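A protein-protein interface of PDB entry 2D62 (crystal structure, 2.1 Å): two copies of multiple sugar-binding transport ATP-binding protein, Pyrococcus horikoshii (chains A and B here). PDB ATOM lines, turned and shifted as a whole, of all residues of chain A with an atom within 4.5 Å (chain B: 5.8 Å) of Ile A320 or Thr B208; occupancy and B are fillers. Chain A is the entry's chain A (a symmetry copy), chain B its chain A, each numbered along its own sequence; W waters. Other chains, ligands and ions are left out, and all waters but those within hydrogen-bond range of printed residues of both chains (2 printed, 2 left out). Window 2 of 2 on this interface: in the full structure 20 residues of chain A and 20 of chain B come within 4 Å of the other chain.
OG1 of Thr B208 lies within hydrogen-bond range of N of Asn A322 (3.0 Å). The side-chain amide nitrogen of Asn A322 sits at hydrogen-bond distance from the backbone carbonyl oxygen of Met B207 (3.4 Å).
The side-chain hydroxyl of Thr B208 lies within hydrogen-bond range of the backbone carbonyl oxygen of Val B204 (2.7 Å). The backbone NH (N) of Glu A321 is in hydrogen-bond range of the backbone carbonyl oxygen (O) of Ile A328, 2.8 Å away. N of Ile A320 is in hydrogen-bond range of OE2 of Glu A350 (3.1 Å).
Among the printed residues, pairs that only touch across the chains: Ile A319 with Ala B183 (3.8 Å), Ile A320 with Thr B208 (3.4 Å), Glu A321 with Thr B208 (3.9 Å), Asn A322 with Val B204 (3.8 Å) and Asn A322 with Pro B227 (3.96 Å).
Of the printed residues of chain B, Ile A319 touches Ala B183. Ile A320 touches just one residue of chain B: Thr B208. Of the printed residues of chain B, Asn A322 touches Val B204, Met B207, Thr B208 and Pro B227. Printed residues of chain A within 4 Å of Met B207: Asn A322 (3.4 Å). Thr B208 touches just these residues of chain A: Ile A320 (3.4 Å), Glu A321 (3.9 Å) and Asn A322 (3.0 Å). The nearest printed residue of chain A that does not touch Thr B208 is Glu A350 (5.7 Å).
Hydrophobic or aromatic side chains of chain A that line the printed part of chain B: Ile A319. Among the printed residues, 7 pairs touch across the chains.
No position is printed for both chains. Of the 7 pairs that touch across the chains among the printed residues, none has its exchanged pair printed and touching as well.
Water W1 lies within hydrogen-bond range of the backbone carbonyl oxygen (O) of Thr B208 (2.8 Å) and the backbone carbonyl oxygen (O) of Ile A320 (3.0 Å). Water W2 bridges ND2 of Asn A322 (3.0 Å) and O of Met B207 (3.0 Å).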
ATOM      1  N   VAL A 317      13.061   3.647 -30.671  1.00  0.00           N
ATOM      2  CA  VAL A 317      11.914   3.551 -29.779  1.00  0.00           C
ATOM      3  C   VAL A 317      11.539   2.099 -29.511  1.00  0.00           C
ATOM      4  O   VAL A 317      11.217   1.356 -30.438  1.00  0.00           O
ATOM      5  CB  VAL A 317      10.692   4.259 -30.388  1.00  0.00           C
ATOM      6  CG1 VAL A 317       9.503   4.155 -29.443  1.00  0.00           C
ATOM      7  CG2 VAL A 317      11.031   5.715 -30.691  1.00  0.00           C
ATOM      8  N   ILE A 319       9.410   1.273 -26.553  1.00  0.00           N
ATOM      9  CA  ILE A 319       8.102   1.284 -25.906  1.00  0.00           C
ATOM     10  C   ILE A 319       7.474   2.669 -25.881  1.00  0.00           C
ATOM     11  O   ILE A 319       8.151   3.671 -25.632  1.00  0.00           O
ATOM     12  CB  ILE A 319       8.195   0.817 -24.432  1.00  0.00           C
ATOM     13  CG1 ILE A 319       8.767  -0.598 -24.355  1.00  0.00           C
ATOM     14  CG2 ILE A 319       6.815   0.887 -23.775  1.00  0.00           C
ATOM     15  CD1 ILE A 319       8.941  -1.104 -22.934  1.00  0.00           C
ATOM     16  N   ILE A 320       6.170   2.716 -26.131  1.00  0.00           N
ATOM     17  CA  ILE A 320       5.441   3.969 -26.092  1.00  0.00           C
ATOM     18  C   ILE A 320       4.237   3.818 -25.189  1.00  0.00           C
ATOM     19  O   ILE A 320       3.341   3.013 -25.459  1.00  0.00           O
ATOM     20  CB  ILE A 320       4.945   4.403 -27.479  1.00  0.00           C
ATOM     21  CG1 ILE A 320       6.133   4.751 -28.378  1.00  0.00           C
ATOM     22  CG2 ILE A 320       4.025   5.611 -27.336  1.00  0.00           C
ATOM     23  CD1 ILE A 320       5.742   5.173 -29.782  1.00  0.00           C
ATOM     24  N   GLU A 321       4.227   4.574 -24.099  1.00  0.00           N
ATOM     25  CA  GLU A 321       3.106   4.552 -23.177  1.00  0.00           C
ATOM     26  C   GLU A 321       2.244   5.750 -23.531  1.00  0.00           C
ATOM     27  O   GLU A 321       2.718   6.887 -23.521  1.00  0.00           O
ATOM     28  CB  GLU A 321       3.574   4.695 -21.732  1.00  0.00           C
ATOM     29  CG  GLU A 321       4.549   3.633 -21.258  1.00  0.00           C
ATOM     30  CD  GLU A 321       4.876   3.799 -19.789  1.00  0.00           C
ATOM     31  OE1 GLU A 321       3.937   3.739 -18.969  1.00  0.00           O
ATOM     32  OE2 GLU A 321       6.063   4.000 -19.453  1.00  0.00           O
ATOM     33  N   ASN A 322       0.983   5.498 -23.855  1.00  0.00           N
ATOM     34  CA  ASN A 322       0.067   6.572 -24.193  1.00  0.00           C
ATOM     35  C   ASN A 322      -0.732   6.909 -22.944  1.00  0.00           C
ATOM     36  O   ASN A 322      -1.687   6.213 -22.612  1.00  0.00           O
ATOM     37  CB  ASN A 322      -0.878   6.137 -25.308  1.00  0.00           C
ATOM     38  CG  ASN A 322      -1.738   7.277 -25.811  1.00  0.00           C
ATOM     39  OD1 ASN A 322      -1.776   8.342 -25.208  1.00  0.00           O
ATOM     40  ND2 ASN A 322      -2.437   7.056 -26.921  1.00  0.00           N
ATOM     41  N   LYS A 327       3.073  11.208 -23.855  1.00  0.00           N
ATOM     42  CA  LYS A 327       3.581   9.890 -24.195  1.00  0.00           C
ATOM     43  C   LYS A 327       4.906   9.654 -23.485  1.00  0.00           C
ATOM     44  O   LYS A 327       5.777  10.523 -23.480  1.00  0.00           O
ATOM     45  CB  LYS A 327       3.798   9.773 -25.707  1.00  0.00           C
ATOM     46  CG  LYS A 327       2.524   9.668 -26.531  1.00  0.00           C
ATOM     47  CD  LYS A 327       2.840   9.701 -28.022  1.00  0.00           C
ATOM     48  CE  LYS A 327       1.610   9.385 -28.871  1.00  0.00           C
ATOM     49  NZ  LYS A 327       0.454  10.255 -28.548  1.00  0.00           N
ATOM     50  N   ILE A 328       5.049   8.489 -22.862  1.00  0.00           N
ATOM     51  CA  ILE A 328       6.293   8.140 -22.193  1.00  0.00           C
ATOM     52  C   ILE A 328       6.997   7.222 -23.181  1.00  0.00           C
ATOM     53  O   ILE A 328       6.497   6.142 -23.510  1.00  0.00           O
ATOM     54  CB  ILE A 328       6.055   7.386 -20.872  1.00  0.00           C
ATOM     55  CG1 ILE A 328       5.193   8.229 -19.925  1.00  0.00           C
ATOM     56  CG2 ILE A 328       7.390   7.046 -20.233  1.00  0.00           C
ATOM     57  CD1 ILE A 328       5.712   9.644 -19.678  1.00  0.00           C
ATOM     58  N   VAL A 348       5.425   9.598 -33.206  1.00  0.00           N
ATOM     59  CA  VAL A 348       6.405   8.533 -33.049  1.00  0.00           C
ATOM     60  C   VAL A 348       5.729   7.168 -32.956  1.00  0.00           C
ATOM     61  O   VAL A 348       4.648   7.033 -32.383  1.00  0.00           O
ATOM     62  CB  VAL A 348       7.259   8.752 -31.782  1.00  0.00           C
ATOM     63  CG1 VAL A 348       6.376   8.716 -30.543  1.00  0.00           C
ATOM     64  CG2 VAL A 348       8.341   7.699 -31.698  1.00  0.00           C
ATOM     65  N   ARG A 349       6.370   6.162 -33.535  1.00  0.00           N
ATOM     66  CA  ARG A 349       5.855   4.799 -33.503  1.00  0.00           C
ATOM     67  C   ARG A 349       6.974   3.879 -33.036  1.00  0.00           C
ATOM     68  O   ARG A 349       8.148   4.157 -33.270  1.00  0.00           O
ATOM     69  CB  ARG A 349       5.375   4.370 -34.892  1.00  0.00           C
ATOM     70  CG  ARG A 349       3.866   4.456 -35.091  1.00  0.00           C
ATOM     71  CD  ARG A 349       3.465   3.878 -36.447  1.00  0.00           C
ATOM     72  NE  ARG A 349       2.048   3.512 -36.516  1.00  0.00           N
ATOM     73  CZ  ARG A 349       1.487   2.531 -35.811  1.00  0.00           C
ATOM     74  NH1 ARG A 349       2.218   1.807 -34.972  1.00  0.00           N
ATOM     75  NH2 ARG A 349       0.194   2.265 -35.952  1.00  0.00           N
ATOM     76  N   GLU A 350       6.615   2.787 -32.373  1.00  0.00           N
ATOM     77  CA  GLU A 350       7.622   1.855 -31.885  1.00  0.00           C
ATOM     78  C   GLU A 350       8.449   1.359 -33.064  1.00  0.00           C
ATOM     79  O   GLU A 350       7.911   1.068 -34.132  1.00  0.00           O
ATOM     80  CB  GLU A 350       6.958   0.684 -31.159  1.00  0.00           C
ATOM     81  CG  GLU A 350       5.857   1.115 -30.189  1.00  0.00           C
ATOM     82  CD  GLU A 350       5.619   0.110 -29.072  1.00  0.00           C
ATOM     83  OE1 GLU A 350       5.977  -1.073 -29.260  1.00  0.00           O
ATOM     84  OE2 GLU A 350       5.069   0.499 -28.014  1.00  0.00           O
ATOM     85  N   ARG B 182       2.773  -4.814 -22.000  1.00  0.00           N
ATOM     86  CA  ARG B 182       1.807  -4.161 -22.885  1.00  0.00           C
ATOM     87  C   ARG B 182       2.441  -4.013 -24.265  1.00  0.00           C
ATOM     88  O   ARG B 182       1.819  -4.304 -25.287  1.00  0.00           O
ATOM     89  CB  ARG B 182       1.434  -2.778 -22.350  1.00  0.00           C
ATOM     90  CG  ARG B 182       0.575  -2.813 -21.104  1.00  0.00           C
ATOM     91  CD  ARG B 182       0.410  -1.427 -20.508  1.00  0.00           C
ATOM     92  NE  ARG B 182      -0.406  -1.463 -19.300  1.00  0.00           N
ATOM     93  CZ  ARG B 182      -0.489  -0.468 -18.427  1.00  0.00           C
ATOM     94  NH1 ARG B 182       0.201   0.649 -18.623  1.00  0.00           N
ATOM     95  NH2 ARG B 182      -1.268  -0.584 -17.362  1.00  0.00           N
ATOM     96  N   ALA B 183       3.694  -3.568 -24.280  1.00  0.00           N
ATOM     97  CA  ALA B 183       4.424  -3.380 -25.527  1.00  0.00           C
ATOM     98  C   ALA B 183       4.741  -4.731 -26.166  1.00  0.00           C
ATOM     99  O   ALA B 183       4.608  -4.909 -27.372  1.00  0.00           O
ATOM    100  CB  ALA B 183       5.717  -2.612 -25.261  1.00  0.00           C
ATOM    101  N   LYS B 186       1.431  -6.319 -27.649  1.00  0.00           N
ATOM    102  CA  LYS B 186       0.993  -5.638 -28.865  1.00  0.00           C
ATOM    103  C   LYS B 186       1.950  -5.898 -30.029  1.00  0.00           C
ATOM    104  O   LYS B 186       1.522  -6.023 -31.174  1.00  0.00           O
ATOM    105  CB  LYS B 186       0.870  -4.129 -28.626  1.00  0.00           C
ATOM    106  CG  LYS B 186       0.383  -3.351 -29.848  1.00  0.00           C
ATOM    107  CD  LYS B 186      -0.927  -3.924 -30.386  1.00  0.00           C
ATOM    108  CE  LYS B 186      -1.374  -3.221 -31.663  1.00  0.00           C
ATOM    109  NZ  LYS B 186      -1.716  -1.780 -31.442  1.00  0.00           N
ATOM    110  N   GLN B 203      -7.514   2.518 -18.395  1.00  0.00           N
ATOM    111  CA  GLN B 203      -7.492   3.460 -19.519  1.00  0.00           C
ATOM    112  C   GLN B 203      -6.143   3.543 -20.225  1.00  0.00           C
ATOM    113  O   GLN B 203      -6.080   3.524 -21.455  1.00  0.00           O
ATOM    114  CB  GLN B 203      -7.891   4.873 -19.056  1.00  0.00           C
ATOM    115  CG  GLN B 203      -9.355   5.029 -18.643  1.00  0.00           C
ATOM    116  CD  GLN B 203      -9.616   4.667 -17.185  1.00  0.00           C
ATOM    117  OE1 GLN B 203      -9.075   3.693 -16.664  1.00  0.00           O
ATOM    118  NE2 GLN B 203     -10.462   5.449 -16.526  1.00  0.00           N
ATOM    119  N   VAL B 204      -5.066   3.642 -19.452  1.00  0.00           N
ATOM    120  CA  VAL B 204      -3.730   3.739 -20.027  1.00  0.00           C
ATOM    121  C   VAL B 204      -3.375   2.501 -20.841  1.00  0.00           C
ATOM    122  O   VAL B 204      -2.807   2.606 -21.930  1.00  0.00           O
ATOM    123  CB  VAL B 204      -2.669   3.954 -18.926  1.00  0.00           C
ATOM    124  CG1 VAL B 204      -1.270   3.918 -19.526  1.00  0.00           C
ATOM    125  CG2 VAL B 204      -2.910   5.294 -18.245  1.00  0.00           C
ATOM    126  N   GLU B 205      -3.709   1.326 -20.319  1.00  0.00           N
ATOM    127  CA  GLU B 205      -3.415   0.096 -21.040  1.00  0.00           C
ATOM    128  C   GLU B 205      -4.209   0.078 -22.350  1.00  0.00           C
ATOM    129  O   GLU B 205      -3.694  -0.311 -23.398  1.00  0.00           O
ATOM    130  CB  GLU B 205      -3.768  -1.121 -20.176  1.00  0.00           C
ATOM    131  CG  GLU B 205      -3.341  -2.448 -20.783  1.00  0.00           C
ATOM    132  CD  GLU B 205      -3.219  -3.552 -19.743  1.00  0.00           C
ATOM    133  OE1 GLU B 205      -2.448  -3.378 -18.773  1.00  0.00           O
ATOM    134  OE2 GLU B 205      -3.888  -4.595 -19.900  1.00  0.00           O
ATOM    135  N   ALA B 206      -5.463   0.520 -22.292  1.00  0.00           N
ATOM    136  CA  ALA B 206      -6.309   0.546 -23.485  1.00  0.00           C
ATOM    137  C   ALA B 206      -5.735   1.499 -24.534  1.00  0.00           C
ATOM    138  O   ALA B 206      -5.541   1.126 -25.691  1.00  0.00           O
ATOM    139  CB  ALA B 206      -7.725   0.969 -23.111  1.00  0.00           C
ATOM    140  N   MET B 207      -5.462   2.727 -24.110  1.00  0.00           N
ATOM    141  CA  MET B 207      -4.909   3.765 -24.978  1.00  0.00           C
ATOM    142  C   MET B 207      -3.561   3.373 -25.565  1.00  0.00           C
ATOM    143  O   MET B 207      -3.225   3.737 -26.689  1.00  0.00           O
ATOM    144  CB  MET B 207      -4.730   5.046 -24.177  1.00  0.00           C
ATOM    145  CG  MET B 207      -6.001   5.553 -23.571  1.00  0.00           C
ATOM    146  SD  MET B 207      -6.903   6.630 -24.847  1.00  0.00           S
ATOM    147  CE  MET B 207      -6.041   8.285 -24.361  1.00  0.00           C
ATOM    148  N   THR B 208      -2.788   2.632 -24.789  1.00  0.00           N
ATOM    149  CA  THR B 208      -1.466   2.207 -25.210  1.00  0.00           C
ATOM    150  C   THR B 208      -1.445   1.081 -26.242  1.00  0.00           C
ATOM    151  O   THR B 208      -0.679   1.128 -27.201  1.00  0.00           O
ATOM    152  CB  THR B 208      -0.641   1.763 -23.983  1.00  0.00           C
ATOM    153  OG1 THR B 208      -0.396   2.898 -23.140  1.00  0.00           O
ATOM    154  CG2 THR B 208       0.687   1.137 -24.416  1.00  0.00           C
ATOM    155  N   MET B 209      -2.300   0.084 -26.054  1.00  0.00           N
ATOM    156  CA  MET B 209      -2.325  -1.089 -26.928  1.00  0.00           C
ATOM    157  C   MET B 209      -3.339  -1.134 -28.066  1.00  0.00           C
ATOM    158  O   MET B 209      -3.064  -1.687 -29.132  1.00  0.00           O
ATOM    159  CB  MET B 209      -2.548  -2.344 -26.074  1.00  0.00           C
ATOM    160  CG  MET B 209      -1.570  -2.544 -24.926  1.00  0.00           C
ATOM    161  SD  MET B 209      -2.061  -4.109 -23.857  1.00  0.00           S
ATOM    162  CE  MET B 209      -1.188  -5.422 -24.944  1.00  0.00           C
ATOM    163  N   GLY B 210      -4.516  -0.572 -27.836  1.00  0.00           N
ATOM    164  CA  GLY B 210      -5.564  -0.651 -28.835  1.00  0.00           C
ATOM    165  C   GLY B 210      -5.474   0.094 -30.150  1.00  0.00           C
ATOM    166  O   GLY B 210      -5.094   1.264 -30.193  1.00  0.00           O
ATOM    167  N   PRO B 227      -7.541   5.521 -30.100  1.00  0.00           N
ATOM    168  CA  PRO B 227      -7.268   6.200 -28.829  1.00  0.00           C
ATOM    169  C   PRO B 227      -7.440   7.720 -28.981  1.00  0.00           C
ATOM    170  O   PRO B 227      -7.990   8.377 -28.103  1.00  0.00           O
ATOM    171  CB  PRO B 227      -5.828   5.805 -28.538  1.00  0.00           C
ATOM    172  CG  PRO B 227      -5.768   4.398 -29.084  1.00  0.00           C
ATOM    173  CD  PRO B 227      -6.502   4.519 -30.402  1.00  0.00           C
HETATM  174  O   HOH W   1       1.283   3.003 -27.691  1.00  0.00           O
HETATM  175  O   HOH W   2      -1.774   5.000 -28.941  1.00  0.00           O
